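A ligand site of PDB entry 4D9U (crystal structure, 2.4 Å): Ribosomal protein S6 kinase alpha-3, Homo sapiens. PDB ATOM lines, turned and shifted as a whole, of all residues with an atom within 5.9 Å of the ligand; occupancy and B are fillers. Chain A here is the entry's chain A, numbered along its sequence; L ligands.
The side-chain sulfur of Cys 38 is covalently linked to a carbon (C8) of the ligand (1.9 Å).
N1 of the ligand lies within hydrogen-bond range of O of Glu 96 (2.7 Å).
OG1 of Thr 95 is in hydrogen-bond range of N1 of the ligand (2.9 Å).
O of Ile 30 is in hydrogen-bond range of O1 of the ligand, 3.1 Å away.
N of Met 98 is in hydrogen-bond range of N5 of the ligand (2.9 Å).
The backbone NH of Cys 38 sits at hydrogen-bond distance from the backbone carbonyl oxygen of Gly 31, at 2.9 Å.
The backbone NH (N) of Thr 95 lies within hydrogen-bond range of the backbone carbonyl oxygen (O) of Ala 51.
The backbone NH of Cys 162 is in hydrogen-bond range of the backbone carbonyl oxygen of Asn 146 (2.8 Å).
The side-chain amino group (NZ) of Lys 53 is in salt-bridge range of the side-chain carboxylate (OD1) of Asp 163.
O of Lys 53 is in hydrogen-bond range of N of Val 93 (2.9 Å).
The backbone NH of Ile 30 is in hydrogen-bond range of the backbone carbonyl oxygen of Cys 38, 2.6 Å away.
The side-chain carboxylate of Glu 65 is in salt-bridge range of the side-chain amino group of Lys 53 (3.1 Å).
Residues that only touch the ligand: Gly 31, Val 32, Gly 33, Ser 36, Val 37, Ala 51, Lys 53, Leu 69, Ile 79, Val 93, Leu 97, Cys 162 and Asp 163.
Hydrophobic or aromatic side chains that line the ligand: Ile 30, Ala 51, Leu 69, Ile 79, Val 93, Leu 97 and Met 98.
18 residues have an atom within 4 Å of the ligand: Ile 30, Gly 31, Val 32, Gly 33, Ser 36, Val 37, Cys 38, Ala 51, Lys 53, Leu 69, Ile 79, Val 93, Thr 95, Glu 96, Leu 97, Met 98, Cys 162 and Asp 163.
The nearest printed residue that does not touch the ligand is Glu 65 (4.1 Å).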
ATOM      1  N   ILE A  30     -20.310 -17.532 -10.064  1.00  0.00           N
ATOM      2  CA  ILE A  30     -20.556 -17.352 -11.484  1.00  0.00           C
ATOM      3  C   ILE A  30     -19.778 -18.378 -12.298  1.00  0.00           C
ATOM      4  O   ILE A  30     -19.827 -18.372 -13.532  1.00  0.00           O
ATOM      5  CB  ILE A  30     -20.242 -15.909 -11.954  1.00  0.00           C
ATOM      6  CG1 ILE A  30     -18.770 -15.554 -11.733  1.00  0.00           C
ATOM      7  CG2 ILE A  30     -21.123 -14.906 -11.205  1.00  0.00           C
ATOM      8  CD1 ILE A  30     -18.455 -14.096 -12.021  1.00  0.00           C
ATOM      9  N   GLY A  31     -19.089 -19.275 -11.608  1.00  0.00           N
ATOM     10  CA  GLY A  31     -18.323 -20.336 -12.253  1.00  0.00           C
ATOM     11  C   GLY A  31     -17.676 -21.209 -11.185  1.00  0.00           C
ATOM     12  O   GLY A  31     -17.277 -20.712 -10.135  1.00  0.00           O
ATOM     13  N   VAL A  32     -17.579 -22.513 -11.434  1.00  0.00           N
ATOM     14  CA  VAL A  32     -17.036 -23.415 -10.424  1.00  0.00           C
ATOM     15  C   VAL A  32     -16.122 -24.495 -11.002  1.00  0.00           C
ATOM     16  O   VAL A  32     -16.359 -25.008 -12.104  1.00  0.00           O
ATOM     17  CB  VAL A  32     -18.147 -24.069  -9.574  1.00  0.00           C
ATOM     18  CG1 VAL A  32     -17.527 -24.943  -8.487  1.00  0.00           C
ATOM     19  CG2 VAL A  32     -19.043 -23.019  -8.954  1.00  0.00           C
ATOM     20  N   GLY A  33     -15.068 -24.809 -10.244  1.00  0.00           N
ATOM     21  CA  GLY A  33     -14.144 -25.888 -10.552  1.00  0.00           C
ATOM     22  C   GLY A  33     -13.729 -26.565  -9.245  1.00  0.00           C
ATOM     23  O   GLY A  33     -14.196 -26.185  -8.176  1.00  0.00           O
ATOM     24  N   SER A  36     -10.974 -24.045  -7.680  1.00  0.00           N
ATOM     25  CA  SER A  36     -11.288 -22.617  -7.677  1.00  0.00           C
ATOM     26  C   SER A  36     -12.739 -22.305  -7.987  1.00  0.00           C
ATOM     27  O   SER A  36     -13.457 -23.137  -8.527  1.00  0.00           O
ATOM     28  CB  SER A  36     -10.342 -21.798  -8.570  1.00  0.00           C
ATOM     29  OG  SER A  36     -10.452 -22.149  -9.935  1.00  0.00           O
ATOM     30  N   VAL A  37     -13.159 -21.100  -7.628  1.00  0.00           N
ATOM     31  CA  VAL A  37     -14.522 -20.627  -7.779  1.00  0.00           C
ATOM     32  C   VAL A  37     -14.516 -19.160  -8.161  1.00  0.00           C
ATOM     33  O   VAL A  37     -13.710 -18.393  -7.631  1.00  0.00           O
ATOM     34  CB  VAL A  37     -15.254 -20.726  -6.439  1.00  0.00           C
ATOM     35  CG1 VAL A  37     -16.767 -20.605  -6.656  1.00  0.00           C
ATOM     36  CG2 VAL A  37     -14.903 -22.017  -5.733  1.00  0.00           C
ATOM     37  N   CYS A  38     -15.401 -18.767  -9.076  1.00  0.00           N
ATOM     38  CA  CYS A  38     -15.579 -17.350  -9.418  1.00  0.00           C
ATOM     39  C   CYS A  38     -16.907 -16.864  -8.849  1.00  0.00           C
ATOM     40  O   CYS A  38     -17.938 -17.443  -9.120  1.00  0.00           O
ATOM     41  CB  CYS A  38     -15.596 -17.139 -10.934  1.00  0.00           C
ATOM     42  SG  CYS A  38     -14.037 -17.469 -11.818  1.00  0.00           S
ATOM     43  N   ALA A  51     -15.637  -9.238 -10.611  1.00  0.00           N
ATOM     44  CA  ALA A  51     -15.538 -10.683 -10.469  1.00  0.00           C
ATOM     45  C   ALA A  51     -14.375 -10.962  -9.538  1.00  0.00           C
ATOM     46  O   ALA A  51     -13.458 -10.148  -9.425  1.00  0.00           O
ATOM     47  CB  ALA A  51     -15.297 -11.334 -11.813  1.00  0.00           C
ATOM     48  N   VAL A  52     -14.411 -12.107  -8.878  1.00  0.00           N
ATOM     49  CA  VAL A  52     -13.315 -12.504  -8.037  1.00  0.00           C
ATOM     50  C   VAL A  52     -13.183 -14.010  -8.079  1.00  0.00           C
ATOM     51  O   VAL A  52     -14.051 -14.744  -7.607  1.00  0.00           O
ATOM     52  CB  VAL A  52     -13.505 -12.032  -6.591  1.00  0.00           C
ATOM     53  CG1 VAL A  52     -14.811 -12.560  -5.995  1.00  0.00           C
ATOM     54  CG2 VAL A  52     -12.310 -12.455  -5.731  1.00  0.00           C
ATOM     55  N   LYS A  53     -12.100 -14.481  -8.681  1.00  0.00           N
ATOM     56  CA  LYS A  53     -11.776 -15.894  -8.659  1.00  0.00           C
ATOM     57  C   LYS A  53     -11.107 -16.155  -7.328  1.00  0.00           C
ATOM     58  O   LYS A  53     -10.139 -15.499  -6.963  1.00  0.00           O
ATOM     59  CB  LYS A  53     -10.867 -16.240  -9.844  1.00  0.00           C
ATOM     60  CG  LYS A  53     -10.281 -17.658  -9.853  1.00  0.00           C
ATOM     61  CD  LYS A  53      -9.723 -17.963 -11.237  1.00  0.00           C
ATOM     62  CE  LYS A  53      -9.134 -19.346 -11.320  1.00  0.00           C
ATOM     63  NZ  LYS A  53      -8.482 -19.594 -12.640  1.00  0.00           N
ATOM     64  N   GLU A  65      -0.467 -17.842 -12.867  1.00  0.00           N
ATOM     65  CA  GLU A  65      -1.619 -17.143 -13.398  1.00  0.00           C
ATOM     66  C   GLU A  65      -1.563 -15.661 -13.008  1.00  0.00           C
ATOM     67  O   GLU A  65      -1.639 -14.785 -13.855  1.00  0.00           O
ATOM     68  CB  GLU A  65      -2.939 -17.779 -12.928  1.00  0.00           C
ATOM     69  CG  GLU A  65      -4.202 -17.062 -13.472  1.00  0.00           C
ATOM     70  CD  GLU A  65      -5.531 -17.707 -13.034  1.00  0.00           C
ATOM     71  OE1 GLU A  65      -5.504 -18.695 -12.270  1.00  0.00           O
ATOM     72  OE2 GLU A  65      -6.612 -17.202 -13.445  1.00  0.00           O
ATOM     73  N   LEU A  69      -1.261 -12.276 -15.304  1.00  0.00           N
ATOM     74  CA  LEU A  69      -2.280 -11.233 -15.240  1.00  0.00           C
ATOM     75  C   LEU A  69      -1.703  -9.875 -14.833  1.00  0.00           C
ATOM     76  O   LEU A  69      -2.133  -8.840 -15.335  1.00  0.00           O
ATOM     77  CB  LEU A  69      -3.416 -11.634 -14.305  1.00  0.00           C
ATOM     78  CG  LEU A  69      -4.397 -12.728 -14.777  1.00  0.00           C
ATOM     79  CD1 LEU A  69      -5.466 -12.899 -13.748  1.00  0.00           C
ATOM     80  CD2 LEU A  69      -4.985 -12.393 -16.121  1.00  0.00           C
ATOM     81  N   ILE A  79      -8.141  -9.902 -19.869  1.00  0.00           N
ATOM     82  CA  ILE A  79      -8.878  -9.579 -18.654  1.00  0.00           C
ATOM     83  C   ILE A  79      -7.991  -8.761 -17.713  1.00  0.00           C
ATOM     84  O   ILE A  79      -6.821  -9.035 -17.583  1.00  0.00           O
ATOM     85  CB  ILE A  79      -9.315 -10.850 -17.924  1.00  0.00           C
ATOM     86  CG1 ILE A  79     -10.079 -10.460 -16.654  1.00  0.00           C
ATOM     87  CG2 ILE A  79      -8.098 -11.727 -17.568  1.00  0.00           C
ATOM     88  CD1 ILE A  79     -10.394 -11.627 -15.751  1.00  0.00           C
ATOM     89  N   LEU A  81      -6.770  -7.177 -14.179  1.00  0.00           N
ATOM     90  CA  LEU A  81      -6.734  -7.410 -12.736  1.00  0.00           C
ATOM     91  C   LEU A  81      -6.881  -6.112 -11.924  1.00  0.00           C
ATOM     92  O   LEU A  81      -6.242  -5.104 -12.237  1.00  0.00           O
ATOM     93  CB  LEU A  81      -5.446  -8.134 -12.364  1.00  0.00           C
ATOM     94  CG  LEU A  81      -5.363  -8.615 -10.916  1.00  0.00           C
ATOM     95  CD1 LEU A  81      -4.855 -10.038 -10.878  1.00  0.00           C
ATOM     96  CD2 LEU A  81      -4.466  -7.686 -10.104  1.00  0.00           C
ATOM     97  N   VAL A  93      -8.436 -13.238  -6.464  1.00  0.00           N
ATOM     98  CA  VAL A  93      -8.049 -12.421  -7.611  1.00  0.00           C
ATOM     99  C   VAL A  93      -9.244 -11.631  -8.158  1.00  0.00           C
ATOM    100  O   VAL A  93     -10.172 -12.190  -8.768  1.00  0.00           O
ATOM    101  CB  VAL A  93      -7.427 -13.280  -8.732  1.00  0.00           C
ATOM    102  CG1 VAL A  93      -6.570 -12.427  -9.648  1.00  0.00           C
ATOM    103  CG2 VAL A  93      -6.604 -14.424  -8.134  1.00  0.00           C
ATOM    104  N   VAL A  94      -9.217 -10.315  -7.933  1.00  0.00           N
ATOM    105  CA  VAL A  94     -10.326  -9.450  -8.308  1.00  0.00           C
ATOM    106  C   VAL A  94     -10.131  -8.879  -9.721  1.00  0.00           C
ATOM    107  O   VAL A  94      -9.105  -8.273 -10.029  1.00  0.00           O
ATOM    108  CB  VAL A  94     -10.467  -8.299  -7.316  1.00  0.00           C
ATOM    109  CG1 VAL A  94     -11.583  -7.358  -7.737  1.00  0.00           C
ATOM    110  CG2 VAL A  94     -10.716  -8.842  -5.928  1.00  0.00           C
ATOM    111  N   THR A  95     -11.126  -9.069 -10.587  1.00  0.00           N
ATOM    112  CA  THR A  95     -11.037  -8.487 -11.919  1.00  0.00           C
ATOM    113  C   THR A  95     -12.245  -7.657 -12.294  1.00  0.00           C
ATOM    114  O   THR A  95     -13.210  -7.546 -11.534  1.00  0.00           O
ATOM    115  CB  THR A  95     -10.826  -9.567 -12.988  1.00  0.00           C
ATOM    116  OG1 THR A  95     -12.023 -10.333 -13.153  1.00  0.00           O
ATOM    117  CG2 THR A  95      -9.671 -10.487 -12.572  1.00  0.00           C
ATOM    118  N   GLU A  96     -12.184  -7.066 -13.479  1.00  0.00           N
ATOM    119  CA  GLU A  96     -13.359  -6.435 -14.083  1.00  0.00           C
ATOM    120  C   GLU A  96     -14.398  -7.540 -14.399  1.00  0.00           C
ATOM    121  O   GLU A  96     -14.042  -8.634 -14.862  1.00  0.00           O
ATOM    122  CB  GLU A  96     -12.970  -5.646 -15.346  1.00  0.00           C
ATOM    123  CG  GLU A  96     -12.262  -6.482 -16.417  1.00  0.00           C
ATOM    124  CD  GLU A  96     -11.806  -5.676 -17.635  1.00  0.00           C
ATOM    125  OE1 GLU A  96     -12.348  -4.567 -17.893  1.00  0.00           O
ATOM    126  OE2 GLU A  96     -10.891  -6.164 -18.343  1.00  0.00           O
ATOM    127  N   LEU A  97     -15.671  -7.248 -14.128  1.00  0.00           N
ATOM    128  CA  LEU A  97     -16.743  -8.209 -14.373  1.00  0.00           C
ATOM    129  C   LEU A  97     -17.251  -8.087 -15.805  1.00  0.00           C
ATOM    130  O   LEU A  97     -17.582  -6.991 -16.265  1.00  0.00           O
ATOM    131  CB  LEU A  97     -17.889  -7.977 -13.395  1.00  0.00           C
ATOM    132  CG  LEU A  97     -19.054  -8.978 -13.485  1.00  0.00           C
ATOM    133  CD1 LEU A  97     -18.672 -10.295 -12.816  1.00  0.00           C
ATOM    134  CD2 LEU A  97     -20.318  -8.391 -12.863  1.00  0.00           C
ATOM    135  N   MET A  98     -17.322  -9.228 -16.487  1.00  0.00           N
ATOM    136  CA  MET A  98     -17.683  -9.301 -17.900  1.00  0.00           C
ATOM    137  C   MET A  98     -19.197  -9.371 -18.078  1.00  0.00           C
ATOM    138  O   MET A  98     -19.836 -10.327 -17.643  1.00  0.00           O
ATOM    139  CB  MET A  98     -17.051 -10.545 -18.541  1.00  0.00           C
ATOM    140  CG  MET A  98     -15.552 -10.661 -18.322  1.00  0.00           C
ATOM    141  SD  MET A  98     -14.610  -9.323 -19.090  1.00  0.00           S
ATOM    142  CE  MET A  98     -13.025  -9.497 -18.241  1.00  0.00           C
ATOM    143  N   LYS A  99     -19.765  -8.378 -18.723  1.00  0.00           N
ATOM    144  CA  LYS A  99     -21.224  -8.281 -18.779  1.00  0.00           C
ATOM    145  C   LYS A  99     -21.822  -8.706 -20.122  1.00  0.00           C
ATOM    146  O   LYS A  99     -23.035  -8.659 -20.291  1.00  0.00           O
ATOM    147  CB  LYS A  99     -21.675  -6.884 -18.364  1.00  0.00           C
ATOM    148  CG  LYS A  99     -21.275  -6.546 -16.935  1.00  0.00           C
ATOM    149  CD  LYS A  99     -21.804  -5.198 -16.503  1.00  0.00           C
ATOM    150  CE  LYS A  99     -22.101  -5.205 -15.008  1.00  0.00           C
ATOM    151  NZ  LYS A  99     -22.876  -4.008 -14.589  1.00  0.00           N
ATOM    152  N   SER A 145     -15.159 -20.791 -24.143  1.00  0.00           N
ATOM    153  CA  SER A 145     -15.762 -20.384 -22.878  1.00  0.00           C
ATOM    154  C   SER A 145     -14.859 -19.493 -22.019  1.00  0.00           C
ATOM    155  O   SER A 145     -15.326 -18.885 -21.050  1.00  0.00           O
ATOM    156  CB  SER A 145     -16.267 -21.583 -22.070  1.00  0.00           C
ATOM    157  OG  SER A 145     -15.353 -22.664 -22.076  1.00  0.00           O
ATOM    158  N   ASN A 146     -13.581 -19.391 -22.386  1.00  0.00           N
ATOM    159  CA  ASN A 146     -12.605 -18.557 -21.666  1.00  0.00           C
ATOM    160  C   ASN A 146     -12.414 -17.206 -22.349  1.00  0.00           C
ATOM    161  O   ASN A 146     -11.580 -16.403 -21.936  1.00  0.00           O
ATOM    162  CB  ASN A 146     -11.246 -19.265 -21.530  1.00  0.00           C
ATOM    163  CG  ASN A 146     -11.331 -20.574 -20.708  1.00  0.00           C
ATOM    164  OD1 ASN A 146     -12.321 -20.827 -20.018  1.00  0.00           O
ATOM    165  ND2 ASN A 146     -10.276 -21.390 -20.782  1.00  0.00           N
ATOM    166  N   LEU A 148     -14.545 -13.840 -23.379  1.00  0.00           N
ATOM    167  CA  LEU A 148     -15.814 -13.177 -23.046  1.00  0.00           C
ATOM    168  C   LEU A 148     -15.884 -11.744 -23.534  1.00  0.00           C
ATOM    169  O   LEU A 148     -14.879 -11.168 -23.952  1.00  0.00           O
ATOM    170  CB  LEU A 148     -16.037 -13.162 -21.528  1.00  0.00           C
ATOM    171  CG  LEU A 148     -15.760 -14.423 -20.724  1.00  0.00           C
ATOM    172  CD1 LEU A 148     -15.635 -14.099 -19.242  1.00  0.00           C
ATOM    173  CD2 LEU A 148     -16.846 -15.464 -20.953  1.00  0.00           C
ATOM    174  N   CYS A 162      -9.899 -14.546 -20.706  1.00  0.00           N
ATOM    175  CA  CYS A 162     -10.235 -14.414 -19.279  1.00  0.00           C
ATOM    176  C   CYS A 162      -9.652 -15.406 -18.277  1.00  0.00           C
ATOM    177  O   CYS A 162      -9.673 -15.131 -17.079  1.00  0.00           O
ATOM    178  CB  CYS A 162     -11.755 -14.394 -19.115  1.00  0.00           C
ATOM    179  SG  CYS A 162     -12.436 -12.845 -19.637  1.00  0.00           S
ATOM    180  N   ASP A 163      -9.206 -16.573 -18.717  1.00  0.00           N
ATOM    181  CA  ASP A 163      -8.627 -17.501 -17.758  1.00  0.00           C
ATOM    182  C   ASP A 163      -7.249 -17.955 -18.177  1.00  0.00           C
ATOM    183  O   ASP A 163      -7.072 -18.544 -19.242  1.00  0.00           O
ATOM    184  CB  ASP A 163      -9.505 -18.733 -17.519  1.00  0.00           C
ATOM    185  CG  ASP A 163      -8.930 -19.639 -16.434  1.00  0.00           C
ATOM    186  OD1 ASP A 163      -9.154 -19.333 -15.240  1.00  0.00           O
ATOM    187  OD2 ASP A 163      -8.238 -20.628 -16.782  1.00  0.00           O
HETATM  188  N1  LIG L   1     -14.145 -11.367 -14.800  1.00  0.00           N
HETATM  189  C1  LIG L   1     -15.137 -12.301 -14.944  1.00  0.00           C
HETATM  190  C2  LIG L   1     -14.927 -13.694 -14.655  1.00  0.00           C
HETATM  191  C3  LIG L   1     -16.101 -14.483 -14.906  1.00  0.00           C
HETATM  192  N2  LIG L   1     -15.856 -15.847 -14.616  1.00  0.00           N
HETATM  193  C4  LIG L   1     -16.966 -16.829 -14.857  1.00  0.00           C
HETATM  194  C5  LIG L   1     -17.228 -17.358 -16.302  1.00  0.00           C
HETATM  195  C6  LIG L   1     -18.242 -18.545 -16.220  1.00  0.00           C
HETATM  196  O1  LIG L   1     -17.753 -19.636 -15.481  1.00  0.00           O
HETATM  197  C7  LIG L   1     -14.487 -15.900 -14.151  1.00  0.00           C
HETATM  198  C8  LIG L   1     -13.643 -17.080 -13.685  1.00  0.00           C
HETATM  199  C9  LIG L   1     -13.961 -18.339 -14.577  1.00  0.00           C
HETATM  200  C10 LIG L   1     -13.348 -19.696 -14.151  1.00  0.00           C
HETATM  201  O2  LIG L   1     -13.750 -20.239 -12.965  1.00  0.00           O
HETATM  202  C11 LIG L   1     -13.274 -21.497 -12.439  1.00  0.00           C
HETATM  203  C12 LIG L   1     -13.789 -22.659 -13.314  1.00  0.00           C
HETATM  204  C13 LIG L   1     -13.799 -21.682 -11.022  1.00  0.00           C
HETATM  205  C14 LIG L   1     -11.744 -21.574 -12.483  1.00  0.00           C
HETATM  206  O3  LIG L   1     -12.534 -20.281 -14.865  1.00  0.00           O
HETATM  207  C15 LIG L   1     -13.435 -18.072 -15.900  1.00  0.00           C
HETATM  208  N3  LIG L   1     -13.031 -17.806 -16.948  1.00  0.00           N
HETATM  209  C16 LIG L   1     -13.910 -14.626 -14.204  1.00  0.00           C
HETATM  210  C17 LIG L   1     -12.507 -14.376 -13.746  1.00  0.00           C
HETATM  211  C18 LIG L   1     -11.353 -14.693 -14.501  1.00  0.00           C
HETATM  212  C19 LIG L   1     -10.062 -14.504 -14.014  1.00  0.00           C
HETATM  213  C20 LIG L   1      -9.822 -14.007 -12.740  1.00  0.00           C
HETATM  214  C21 LIG L   1      -8.463 -13.780 -12.157  1.00  0.00           C
HETATM  215  C22 LIG L   1     -10.945 -13.696 -11.973  1.00  0.00           C
HETATM  216  C23 LIG L   1     -12.238 -13.891 -12.452  1.00  0.00           C
HETATM  217  N4  LIG L   1     -17.321 -14.011 -15.394  1.00  0.00           N
HETATM  218  C24 LIG L   1     -17.344 -12.678 -15.603  1.00  0.00           C
HETATM  219  N5  LIG L   1     -16.341 -11.791 -15.417  1.00  0.00           N
